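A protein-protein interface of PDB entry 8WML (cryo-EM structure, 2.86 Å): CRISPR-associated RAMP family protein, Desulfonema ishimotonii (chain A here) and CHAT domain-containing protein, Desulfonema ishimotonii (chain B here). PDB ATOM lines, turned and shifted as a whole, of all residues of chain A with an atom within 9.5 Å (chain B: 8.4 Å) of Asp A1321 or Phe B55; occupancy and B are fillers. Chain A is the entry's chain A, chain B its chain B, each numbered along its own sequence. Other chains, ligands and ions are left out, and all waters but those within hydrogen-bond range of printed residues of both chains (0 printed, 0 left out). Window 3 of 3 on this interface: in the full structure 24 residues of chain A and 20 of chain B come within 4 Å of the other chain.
The side-chain carboxylate (OE1) of Glu A1318 is in salt-bridge range of the guanidinium group (NE) of Arg B51.
OE1 of Glu A1330 is in salt-bridge range of NH2 of Arg B62, at 2.9 Å.
O of Leu A1333 is in hydrogen-bond range of N of Leu B48, 3.1 Å away.
O of Leu A1334 is in hydrogen-bond range of NH1 of Arg B51 (2.9 Å).
NE1 of Trp A1316 sits at hydrogen-bond distance from O of Glu A1318.
The backbone NH of Ser A1323 sits close to the side-chain carboxylate of Asp A1321, at 3.3 Å.
O of Leu A1322 lies close to OD1 of Asn A1326, at 2.9 Å.
O of Phe B55 lies within hydrogen-bond range of OG of Ser B59.
Hydrophobic or aromatic side chains of chain A that line the printed part of chain B: Leu A1322 and Leu A1325.
Among the printed residues, 8 pairs touch across the chains.
Of the printed residues of chain B, Leu A1322 touches Phe B55 (3.7 Å).
Printed residues of chain B within 4 Å of Leu A1325: Phe B55 and Leu B58.
Of the printed residues of chain B, Leu A1333 touches Leu B48.
Printed residues of chain A within 4 Å of Arg B51: Glu A1318 and Leu A1334.
No residue of chain A comes within 4 Å of Ser B56.
Gln B57 touches none of the printed residues of chain A.
Of the printed residues of chain A, Leu B58 touches Leu A1325 (3.96 Å).
The nearest printed residue of chain A that does not touch Phe B55 is Leu A1334 (4.2 Å).
The nearest printed residue of chain B that does not touch Leu A1333 is Arg B51 (4.5 Å).
Asp A1321 touches Phe B55.
Leu A1322 touches Phe B55.
CD1 of Leu A1325 touches CD1 of Phe B55, at 3.5 Å.
CD2 of Leu A1325 touches O of Leu B58, 3.96 Å away.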
ATOM      1  N   LYS A 277      21.795   0.394  17.531  1.00  0.00           N
ATOM      2  CA  LYS A 277      20.670   1.247  17.152  1.00  0.00           C
ATOM      3  C   LYS A 277      19.368   0.602  17.593  1.00  0.00           C
ATOM      4  O   LYS A 277      18.313   0.836  16.993  1.00  0.00           O
ATOM      5  CB  LYS A 277      20.639   1.494  15.640  1.00  0.00           C
ATOM      6  CG  LYS A 277      21.800   2.320  15.109  1.00  0.00           C
ATOM      7  CD  LYS A 277      21.704   2.495  13.593  1.00  0.00           C
ATOM      8  CE  LYS A 277      22.844   3.339  13.033  1.00  0.00           C
ATOM      9  NZ  LYS A 277      22.771   3.495  11.547  1.00  0.00           N
ATOM     10  N   MET A1300      15.551  -1.243  -6.584  1.00  0.00           N
ATOM     11  CA  MET A1300      15.159  -2.426  -5.833  1.00  0.00           C
ATOM     12  C   MET A1300      14.109  -3.214  -6.612  1.00  0.00           C
ATOM     13  O   MET A1300      13.525  -2.734  -7.585  1.00  0.00           O
ATOM     14  CB  MET A1300      14.621  -2.054  -4.449  1.00  0.00           C
ATOM     15  CG  MET A1300      15.271  -0.843  -3.791  1.00  0.00           C
ATOM     16  SD  MET A1300      14.743  -0.636  -2.081  1.00  0.00           S
ATOM     17  CE  MET A1300      15.862   0.646  -1.528  1.00  0.00           C
ATOM     18  N   ASP A1315       6.210  -1.148   2.198  1.00  0.00           N
ATOM     19  CA  ASP A1315       7.456  -0.645   2.758  1.00  0.00           C
ATOM     20  C   ASP A1315       7.964   0.517   1.915  1.00  0.00           C
ATOM     21  O   ASP A1315       7.502   0.756   0.797  1.00  0.00           O
ATOM     22  CB  ASP A1315       8.520  -1.751   2.825  1.00  0.00           C
ATOM     23  CG  ASP A1315       8.321  -2.693   4.000  1.00  0.00           C
ATOM     24  OD1 ASP A1315       7.487  -2.401   4.883  1.00  0.00           O
ATOM     25  OD2 ASP A1315       9.007  -3.736   4.042  1.00  0.00           O
ATOM     26  N   TRP A1316       8.931   1.243   2.472  1.00  0.00           N
ATOM     27  CA  TRP A1316       9.510   2.401   1.805  1.00  0.00           C
ATOM     28  C   TRP A1316      10.545   1.953   0.781  1.00  0.00           C
ATOM     29  O   TRP A1316      11.489   1.232   1.117  1.00  0.00           O
ATOM     30  CB  TRP A1316      10.152   3.326   2.835  1.00  0.00           C
ATOM     31  CG  TRP A1316      10.528   4.673   2.309  1.00  0.00           C
ATOM     32  CD1 TRP A1316      11.789   5.168   2.152  1.00  0.00           C
ATOM     33  CD2 TRP A1316       9.635   5.707   1.880  1.00  0.00           C
ATOM     34  NE1 TRP A1316      11.737   6.445   1.649  1.00  0.00           N
ATOM     35  CE2 TRP A1316      10.426   6.799   1.473  1.00  0.00           C
ATOM     36  CE3 TRP A1316       8.244   5.814   1.799  1.00  0.00           C
ATOM     37  CZ2 TRP A1316       9.873   7.982   0.992  1.00  0.00           C
ATOM     38  CZ3 TRP A1316       7.698   6.989   1.322  1.00  0.00           C
ATOM     39  CH2 TRP A1316       8.510   8.058   0.926  1.00  0.00           C
ATOM     40  N   VAL A1317      10.370   2.392  -0.467  1.00  0.00           N
ATOM     41  CA  VAL A1317      11.245   2.010  -1.572  1.00  0.00           C
ATOM     42  C   VAL A1317      11.983   3.237  -2.098  1.00  0.00           C
ATOM     43  O   VAL A1317      13.088   3.122  -2.638  1.00  0.00           O
ATOM     44  CB  VAL A1317      10.443   1.325  -2.695  1.00  0.00           C
ATOM     45  CG1 VAL A1317      11.314   1.110  -3.927  1.00  0.00           C
ATOM     46  CG2 VAL A1317       9.874   0.005  -2.208  1.00  0.00           C
ATOM     47  N   GLU A1318      11.390   4.416  -1.940  1.00  0.00           N
ATOM     48  CA  GLU A1318      11.974   5.625  -2.496  1.00  0.00           C
ATOM     49  C   GLU A1318      13.196   6.050  -1.682  1.00  0.00           C
ATOM     50  O   GLU A1318      13.481   5.523  -0.603  1.00  0.00           O
ATOM     51  CB  GLU A1318      10.944   6.762  -2.561  1.00  0.00           C
ATOM     52  CG  GLU A1318       9.693   6.554  -3.463  1.00  0.00           C
ATOM     53  CD  GLU A1318       8.775   5.393  -3.083  1.00  0.00           C
ATOM     54  OE1 GLU A1318       7.624   5.369  -3.566  1.00  0.00           O
ATOM     55  OE2 GLU A1318       9.193   4.509  -2.310  1.00  0.00           O
ATOM     56  N   ASP A1319      13.927   7.023  -2.222  1.00  0.00           N
ATOM     57  CA  ASP A1319      15.164   7.494  -1.611  1.00  0.00           C
ATOM     58  C   ASP A1319      14.824   8.319  -0.377  1.00  0.00           C
ATOM     59  O   ASP A1319      14.297   9.430  -0.489  1.00  0.00           O
ATOM     60  CB  ASP A1319      15.979   8.309  -2.611  1.00  0.00           C
ATOM     61  CG  ASP A1319      16.137   7.609  -3.945  1.00  0.00           C
ATOM     62  OD1 ASP A1319      15.584   6.501  -4.107  1.00  0.00           O
ATOM     63  OD2 ASP A1319      16.817   8.165  -4.833  1.00  0.00           O
ATOM     64  N   GLY A1320      15.125   7.775   0.797  1.00  0.00           N
ATOM     65  CA  GLY A1320      14.850   8.457   2.044  1.00  0.00           C
ATOM     66  C   GLY A1320      14.906   7.515   3.227  1.00  0.00           C
ATOM     67  O   GLY A1320      14.442   6.374   3.143  1.00  0.00           O
ATOM     68  N   ASP A1321      15.474   7.980   4.340  1.00  0.00           N
ATOM     69  CA  ASP A1321      15.587   7.123   5.514  1.00  0.00           C
ATOM     70  C   ASP A1321      14.227   6.869   6.155  1.00  0.00           C
ATOM     71  O   ASP A1321      13.976   5.776   6.676  1.00  0.00           O
ATOM     72  CB  ASP A1321      16.567   7.735   6.521  1.00  0.00           C
ATOM     73  CG  ASP A1321      16.113   9.092   7.050  1.00  0.00           C
ATOM     74  OD1 ASP A1321      15.059   9.602   6.618  1.00  0.00           O
ATOM     75  OD2 ASP A1321      16.824   9.650   7.913  1.00  0.00           O
ATOM     76  N   LEU A1322      13.343   7.867   6.134  1.00  0.00           N
ATOM     77  CA  LEU A1322      12.019   7.819   6.750  1.00  0.00           C
ATOM     78  C   LEU A1322      12.077   7.760   8.272  1.00  0.00           C
ATOM     79  O   LEU A1322      11.044   7.531   8.913  1.00  0.00           O
ATOM     80  CB  LEU A1322      11.196   6.634   6.227  1.00  0.00           C
ATOM     81  CG  LEU A1322       9.669   6.761   6.272  1.00  0.00           C
ATOM     82  CD1 LEU A1322       9.162   7.713   5.204  1.00  0.00           C
ATOM     83  CD2 LEU A1322       9.016   5.397   6.128  1.00  0.00           C
ATOM     84  N   SER A1323      13.251   7.965   8.874  1.00  0.00           N
ATOM     85  CA  SER A1323      13.389   7.934  10.323  1.00  0.00           C
ATOM     86  C   SER A1323      13.168   9.293  10.970  1.00  0.00           C
ATOM     87  O   SER A1323      12.909   9.353  12.177  1.00  0.00           O
ATOM     88  CB  SER A1323      14.777   7.413  10.707  1.00  0.00           C
ATOM     89  OG  SER A1323      14.948   6.072  10.282  1.00  0.00           O
ATOM     90  N   ALA A1324      13.261  10.382  10.202  1.00  0.00           N
ATOM     91  CA  ALA A1324      13.007  11.705  10.762  1.00  0.00           C
ATOM     92  C   ALA A1324      11.558  11.843  11.210  1.00  0.00           C
ATOM     93  O   ALA A1324      11.272  12.508  12.212  1.00  0.00           O
ATOM     94  CB  ALA A1324      13.356  12.785   9.739  1.00  0.00           C
ATOM     95  N   LEU A1325      10.634  11.220  10.483  1.00  0.00           N
ATOM     96  CA  LEU A1325       9.214  11.279  10.798  1.00  0.00           C
ATOM     97  C   LEU A1325       8.784  10.210  11.799  1.00  0.00           C
ATOM     98  O   LEU A1325       7.585  10.069  12.054  1.00  0.00           O
ATOM     99  CB  LEU A1325       8.391  11.149   9.513  1.00  0.00           C
ATOM    100  CG  LEU A1325       8.467  12.346   8.560  1.00  0.00           C
ATOM    101  CD1 LEU A1325       7.979  11.958   7.174  1.00  0.00           C
ATOM    102  CD2 LEU A1325       7.674  13.528   9.093  1.00  0.00           C
ATOM    103  N   ASN A1326       9.725   9.458  12.369  1.00  0.00           N
ATOM    104  CA  ASN A1326       9.381   8.508  13.415  1.00  0.00           C
ATOM    105  C   ASN A1326       8.852   9.241  14.642  1.00  0.00           C
ATOM    106  O   ASN A1326       9.156  10.413  14.882  1.00  0.00           O
ATOM    107  CB  ASN A1326      10.594   7.661  13.794  1.00  0.00           C
ATOM    108  CG  ASN A1326      10.939   6.630  12.740  1.00  0.00           C
ATOM    109  OD1 ASN A1326      10.441   6.685  11.615  1.00  0.00           O
ATOM    110  ND2 ASN A1326      11.795   5.682  13.097  1.00  0.00           N
ATOM    111  N   GLU A1330       1.625  11.063  11.396  1.00  0.00           N
ATOM    112  CA  GLU A1330       1.412  11.120   9.955  1.00  0.00           C
ATOM    113  C   GLU A1330       2.377  10.246   9.164  1.00  0.00           C
ATOM    114  O   GLU A1330       2.212  10.128   7.945  1.00  0.00           O
ATOM    115  CB  GLU A1330       1.484  12.577   9.464  1.00  0.00           C
ATOM    116  CG  GLU A1330       2.873  13.250   9.401  1.00  0.00           C
ATOM    117  CD  GLU A1330       3.388  13.702  10.753  1.00  0.00           C
ATOM    118  OE1 GLU A1330       2.692  13.484  11.767  1.00  0.00           O
ATOM    119  OE2 GLU A1330       4.491  14.287  10.802  1.00  0.00           O
ATOM    120  N   LYS A1331       3.373   9.638   9.811  1.00  0.00           N
ATOM    121  CA  LYS A1331       4.307   8.788   9.083  1.00  0.00           C
ATOM    122  C   LYS A1331       3.617   7.567   8.487  1.00  0.00           C
ATOM    123  O   LYS A1331       4.037   7.078   7.433  1.00  0.00           O
ATOM    124  CB  LYS A1331       5.441   8.353  10.010  1.00  0.00           C
ATOM    125  CG  LYS A1331       6.604   7.673   9.308  1.00  0.00           C
ATOM    126  CD  LYS A1331       7.621   7.174  10.316  1.00  0.00           C
ATOM    127  CE  LYS A1331       7.436   5.700  10.635  1.00  0.00           C
ATOM    128  NZ  LYS A1331       8.179   4.832   9.684  1.00  0.00           N
ATOM    129  N   LEU A1333       0.811   7.352   7.012  1.00  0.00           N
ATOM    130  CA  LEU A1333       0.122   7.645   5.761  1.00  0.00           C
ATOM    131  C   LEU A1333       1.041   7.582   4.549  1.00  0.00           C
ATOM    132  O   LEU A1333       0.540   7.558   3.421  1.00  0.00           O
ATOM    133  CB  LEU A1333      -0.533   9.026   5.831  1.00  0.00           C
ATOM    134  CG  LEU A1333      -1.539   9.266   6.959  1.00  0.00           C
ATOM    135  CD1 LEU A1333      -2.075  10.684   6.885  1.00  0.00           C
ATOM    136  CD2 LEU A1333      -2.681   8.261   6.912  1.00  0.00           C
ATOM    137  N   LEU A1334       2.359   7.555   4.747  1.00  0.00           N
ATOM    138  CA  LEU A1334       3.304   7.445   3.644  1.00  0.00           C
ATOM    139  C   LEU A1334       3.555   6.006   3.211  1.00  0.00           C
ATOM    140  O   LEU A1334       4.351   5.793   2.292  1.00  0.00           O
ATOM    141  CB  LEU A1334       4.634   8.098   4.029  1.00  0.00           C
ATOM    142  CG  LEU A1334       4.591   9.614   4.228  1.00  0.00           C
ATOM    143  CD1 LEU A1334       5.745  10.071   5.106  1.00  0.00           C
ATOM    144  CD2 LEU A1334       4.621  10.331   2.889  1.00  0.00           C
ATOM    145  N   LEU A1335       2.906   5.024   3.845  1.00  0.00           N
ATOM    146  CA  LEU A1335       3.087   3.611   3.524  1.00  0.00           C
ATOM    147  C   LEU A1335       1.804   2.941   3.045  1.00  0.00           C
ATOM    148  O   LEU A1335       1.776   1.711   2.924  1.00  0.00           O
ATOM    149  CB  LEU A1335       3.635   2.860   4.743  1.00  0.00           C
ATOM    150  CG  LEU A1335       4.970   3.339   5.321  1.00  0.00           C
ATOM    151  CD1 LEU A1335       5.039   3.055   6.809  1.00  0.00           C
ATOM    152  CD2 LEU A1335       6.135   2.684   4.604  1.00  0.00           C
ATOM    153  N   LEU B  10      -1.322  20.053   1.833  1.00  0.00           N
ATOM    154  CA  LEU B  10       0.081  19.781   1.424  1.00  0.00           C
ATOM    155  C   LEU B  10       0.315  20.247  -0.015  1.00  0.00           C
ATOM    156  O   LEU B  10       1.245  21.029  -0.233  1.00  0.00           O
ATOM    157  CB  LEU B  10       0.350  18.279   1.547  1.00  0.00           C
ATOM    158  CG  LEU B  10       1.077  17.840   2.816  1.00  0.00           C
ATOM    159  CD1 LEU B  10       1.801  16.523   2.591  1.00  0.00           C
ATOM    160  CD2 LEU B  10       2.053  18.910   3.277  1.00  0.00           C
ATOM    161  N   PHE B  15       5.766  27.458   2.557  1.00  0.00           N
ATOM    162  CA  PHE B  15       6.173  27.645   3.945  1.00  0.00           C
ATOM    163  C   PHE B  15       6.417  29.099   4.329  1.00  0.00           C
ATOM    164  O   PHE B  15       6.694  29.364   5.504  1.00  0.00           O
ATOM    165  CB  PHE B  15       7.434  26.824   4.260  1.00  0.00           C
ATOM    166  CG  PHE B  15       7.184  25.341   4.436  1.00  0.00           C
ATOM    167  CD1 PHE B  15       6.351  24.630   3.582  1.00  0.00           C
ATOM    168  CD2 PHE B  15       7.823  24.651   5.452  1.00  0.00           C
ATOM    169  CE1 PHE B  15       6.142  23.281   3.755  1.00  0.00           C
ATOM    170  CE2 PHE B  15       7.606  23.302   5.632  1.00  0.00           C
ATOM    171  CZ  PHE B  15       6.772  22.616   4.778  1.00  0.00           C
ATOM    172  N   LEU B  48      -1.273   9.168   1.423  1.00  0.00           N
ATOM    173  CA  LEU B  48      -1.060  10.336   0.583  1.00  0.00           C
ATOM    174  C   LEU B  48      -0.465   9.941  -0.767  1.00  0.00           C
ATOM    175  O   LEU B  48       0.087   8.852  -0.939  1.00  0.00           O
ATOM    176  CB  LEU B  48      -0.137  11.335   1.283  1.00  0.00           C
ATOM    177  CG  LEU B  48      -0.416  11.602   2.764  1.00  0.00           C
ATOM    178  CD1 LEU B  48       0.478  12.718   3.275  1.00  0.00           C
ATOM    179  CD2 LEU B  48      -1.880  11.945   2.992  1.00  0.00           C
ATOM    180  N   SER B  49      -0.589  10.853  -1.729  1.00  0.00           N
ATOM    181  CA  SER B  49      -0.014  10.710  -3.058  1.00  0.00           C
ATOM    182  C   SER B  49       1.216  11.603  -3.194  1.00  0.00           C
ATOM    183  O   SER B  49       1.465  12.488  -2.373  1.00  0.00           O
ATOM    184  CB  SER B  49      -1.047  11.061  -4.132  1.00  0.00           C
ATOM    185  OG  SER B  49      -2.168  10.199  -4.064  1.00  0.00           O
ATOM    186  N   ASN B  50       1.981  11.366  -4.263  1.00  0.00           N
ATOM    187  CA  ASN B  50       3.237  12.074  -4.523  1.00  0.00           C
ATOM    188  C   ASN B  50       4.179  11.928  -3.322  1.00  0.00           C
ATOM    189  O   ASN B  50       4.460  12.868  -2.575  1.00  0.00           O
ATOM    190  CB  ASN B  50       2.963  13.550  -4.877  1.00  0.00           C
ATOM    191  CG  ASN B  50       3.248  13.887  -6.342  1.00  0.00           C
ATOM    192  OD1 ASN B  50       3.968  13.176  -7.046  1.00  0.00           O
ATOM    193  ND2 ASN B  50       2.678  14.995  -6.799  1.00  0.00           N
ATOM    194  N   ARG B  51       4.619  10.682  -3.131  1.00  0.00           N
ATOM    195  CA  ARG B  51       5.390  10.339  -1.939  1.00  0.00           C
ATOM    196  C   ARG B  51       6.661  11.163  -1.752  1.00  0.00           C
ATOM    197  O   ARG B  51       6.907  11.595  -0.614  1.00  0.00           O
ATOM    198  CB  ARG B  51       5.732   8.845  -1.947  1.00  0.00           C
ATOM    199  CG  ARG B  51       4.529   7.926  -1.902  1.00  0.00           C
ATOM    200  CD  ARG B  51       4.973   6.493  -1.687  1.00  0.00           C
ATOM    201  NE  ARG B  51       3.944   5.521  -2.037  1.00  0.00           N
ATOM    202  CZ  ARG B  51       2.914   5.190  -1.270  1.00  0.00           C
ATOM    203  NH1 ARG B  51       2.705   5.764  -0.096  1.00  0.00           N
ATOM    204  NH2 ARG B  51       2.066   4.257  -1.694  1.00  0.00           N
ATOM    205  N   PRO B  52       7.505  11.405  -2.764  1.00  0.00           N
ATOM    206  CA  PRO B  52       8.718  12.204  -2.494  1.00  0.00           C
ATOM    207  C   PRO B  52       8.414  13.626  -2.056  1.00  0.00           C
ATOM    208  O   PRO B  52       8.993  14.112  -1.073  1.00  0.00           O
ATOM    209  CB  PRO B  52       9.475  12.163  -3.832  1.00  0.00           C
ATOM    210  CG  PRO B  52       8.854  11.076  -4.621  1.00  0.00           C
ATOM    211  CD  PRO B  52       7.440  10.988  -4.176  1.00  0.00           C
ATOM    212  N   ASN B  53       7.513  14.310  -2.764  1.00  0.00           N
ATOM    213  CA  ASN B  53       7.182  15.684  -2.406  1.00  0.00           C
ATOM    214  C   ASN B  53       6.517  15.743  -1.035  1.00  0.00           C
ATOM    215  O   ASN B  53       6.815  16.634  -0.228  1.00  0.00           O
ATOM    216  CB  ASN B  53       6.274  16.291  -3.480  1.00  0.00           C
ATOM    217  CG  ASN B  53       5.868  17.735  -3.188  1.00  0.00           C
ATOM    218  OD1 ASN B  53       4.782  18.159  -3.581  1.00  0.00           O
ATOM    219  ND2 ASN B  53       6.756  18.513  -2.568  1.00  0.00           N
ATOM    220  N   SER B  54       5.619  14.796  -0.752  1.00  0.00           N
ATOM    221  CA  SER B  54       4.957  14.756   0.549  1.00  0.00           C
ATOM    222  C   SER B  54       5.957  14.510   1.670  1.00  0.00           C
ATOM    223  O   SER B  54       5.885  15.151   2.724  1.00  0.00           O
ATOM    224  CB  SER B  54       3.876  13.675   0.556  1.00  0.00           C
ATOM    225  OG  SER B  54       3.020  13.794  -0.565  1.00  0.00           O
ATOM    226  N   PHE B  55       6.892  13.579   1.466  1.00  0.00           N
ATOM    227  CA  PHE B  55       7.918  13.324   2.471  1.00  0.00           C
ATOM    228  C   PHE B  55       8.774  14.556   2.705  1.00  0.00           C
ATOM    229  O   PHE B  55       9.066  14.907   3.855  1.00  0.00           O
ATOM    230  CB  PHE B  55       8.787  12.145   2.040  1.00  0.00           C
ATOM    231  CG  PHE B  55       9.942  11.876   2.960  1.00  0.00           C
ATOM    232  CD1 PHE B  55       9.746  11.289   4.196  1.00  0.00           C
ATOM    233  CD2 PHE B  55      11.231  12.210   2.581  1.00  0.00           C
ATOM    234  CE1 PHE B  55      10.814  11.047   5.038  1.00  0.00           C
ATOM    235  CE2 PHE B  55      12.299  11.969   3.418  1.00  0.00           C
ATOM    236  CZ  PHE B  55      12.090  11.385   4.646  1.00  0.00           C
ATOM    237  N   SER B  56       9.174  15.238   1.629  1.00  0.00           N
ATOM    238  CA  SER B  56       9.990  16.438   1.778  1.00  0.00           C
ATOM    239  C   SER B  56       9.244  17.510   2.563  1.00  0.00           C
ATOM    240  O   SER B  56       9.793  18.113   3.493  1.00  0.00           O
ATOM    241  CB  SER B  56      10.399  16.968   0.404  1.00  0.00           C
ATOM    242  OG  SER B  56      11.083  18.203   0.520  1.00  0.00           O
ATOM    243  N   GLN B  57       7.972  17.736   2.222  1.00  0.00           N
ATOM    244  CA  GLN B  57       7.213  18.787   2.893  1.00  0.00           C
ATOM    245  C   GLN B  57       6.960  18.443   4.356  1.00  0.00           C
ATOM    246  O   GLN B  57       7.077  19.311   5.226  1.00  0.00           O
ATOM    247  CB  GLN B  57       5.888  19.038   2.174  1.00  0.00           C
ATOM    248  CG  GLN B  57       5.904  20.276   1.296  1.00  0.00           C
ATOM    249  CD  GLN B  57       4.638  20.431   0.485  1.00  0.00           C
ATOM    250  OE1 GLN B  57       3.744  21.188   0.858  1.00  0.00           O
ATOM    251  NE2 GLN B  57       4.543  19.701  -0.617  1.00  0.00           N
ATOM    252  N   LEU B  58       6.598  17.191   4.649  1.00  0.00           N
ATOM    253  CA  LEU B  58       6.350  16.809   6.034  1.00  0.00           C
ATOM    254  C   LEU B  58       7.624  16.887   6.866  1.00  0.00           C
ATOM    255  O   LEU B  58       7.590  17.336   8.017  1.00  0.00           O
ATOM    256  CB  LEU B  58       5.753  15.403   6.099  1.00  0.00           C
ATOM    257  CG  LEU B  58       4.330  15.229   5.558  1.00  0.00           C
ATOM    258  CD1 LEU B  58       3.954  13.755   5.498  1.00  0.00           C
ATOM    259  CD2 LEU B  58       3.322  15.997   6.399  1.00  0.00           C
ATOM    260  N   SER B  59       8.757  16.451   6.308  1.00  0.00           N
ATOM    261  CA  SER B  59      10.019  16.558   7.029  1.00  0.00           C
ATOM    262  C   SER B  59      10.377  18.014   7.284  1.00  0.00           C
ATOM    263  O   SER B  59      10.857  18.362   8.369  1.00  0.00           O
ATOM    264  CB  SER B  59      11.133  15.867   6.245  1.00  0.00           C
ATOM    265  OG  SER B  59      11.401  16.558   5.038  1.00  0.00           O
ATOM    266  N   GLN B  60      10.152  18.880   6.295  1.00  0.00           N
ATOM    267  CA  GLN B  60      10.429  20.300   6.478  1.00  0.00           C
ATOM    268  C   GLN B  60       9.527  20.911   7.549  1.00  0.00           C
ATOM    269  O   GLN B  60       9.985  21.716   8.368  1.00  0.00           O
ATOM    270  CB  GLN B  60      10.265  21.020   5.139  1.00  0.00           C
ATOM    271  CG  GLN B  60      11.037  22.335   5.015  1.00  0.00           C
ATOM    272  CD  GLN B  60      11.358  22.747   3.572  1.00  0.00           C
ATOM    273  OE1 GLN B  60      12.308  23.496   3.344  1.00  0.00           O
ATOM    274  NE2 GLN B  60      10.561  22.291   2.601  1.00  0.00           N
ATOM    275  N   PHE B  61       8.243  20.545   7.555  1.00  0.00           N
ATOM    276  CA  PHE B  61       7.322  21.060   8.567  1.00  0.00           C
ATOM    277  C   PHE B  61       7.701  20.590   9.965  1.00  0.00           C
ATOM    278  O   PHE B  61       7.727  21.388  10.909  1.00  0.00           O
ATOM    279  CB  PHE B  61       5.890  20.642   8.231  1.00  0.00           C
ATOM    280  CG  PHE B  61       4.839  21.432   8.959  1.00  0.00           C
ATOM    281  CD1 PHE B  61       4.432  21.061  10.230  1.00  0.00           C
ATOM    282  CD2 PHE B  61       4.260  22.544   8.376  1.00  0.00           C
ATOM    283  CE1 PHE B  61       3.466  21.781  10.902  1.00  0.00           C
ATOM    284  CE2 PHE B  61       3.290  23.269   9.047  1.00  0.00           C
ATOM    285  CZ  PHE B  61       2.896  22.885  10.310  1.00  0.00           C
ATOM    286  N   ARG B  62       7.823  19.285  10.171  1.00  0.00           N
ATOM    287  CA  ARG B  62       8.059  18.786  11.554  1.00  0.00           C
ATOM    288  C   ARG B  62       9.505  19.075  11.963  1.00  0.00           C
ATOM    289  O   ARG B  62       9.902  18.616  13.046  1.00  0.00           O
ATOM    290  CB  ARG B  62       7.675  17.308  11.697  1.00  0.00           C
ATOM    291  CG  ARG B  62       6.191  17.040  11.515  1.00  0.00           C
ATOM    292  CD  ARG B  62       5.413  17.263  12.794  1.00  0.00           C
ATOM    293  NE  ARG B  62       4.254  16.386  12.862  1.00  0.00           N
ATOM    294  CZ  ARG B  62       3.376  16.376  13.856  1.00  0.00           C
ATOM    295  NH1 ARG B  62       3.527  17.202  14.876  1.00  0.00           N
ATOM    296  NH2 ARG B  62       2.352  15.541  13.829  1.00  0.00           N
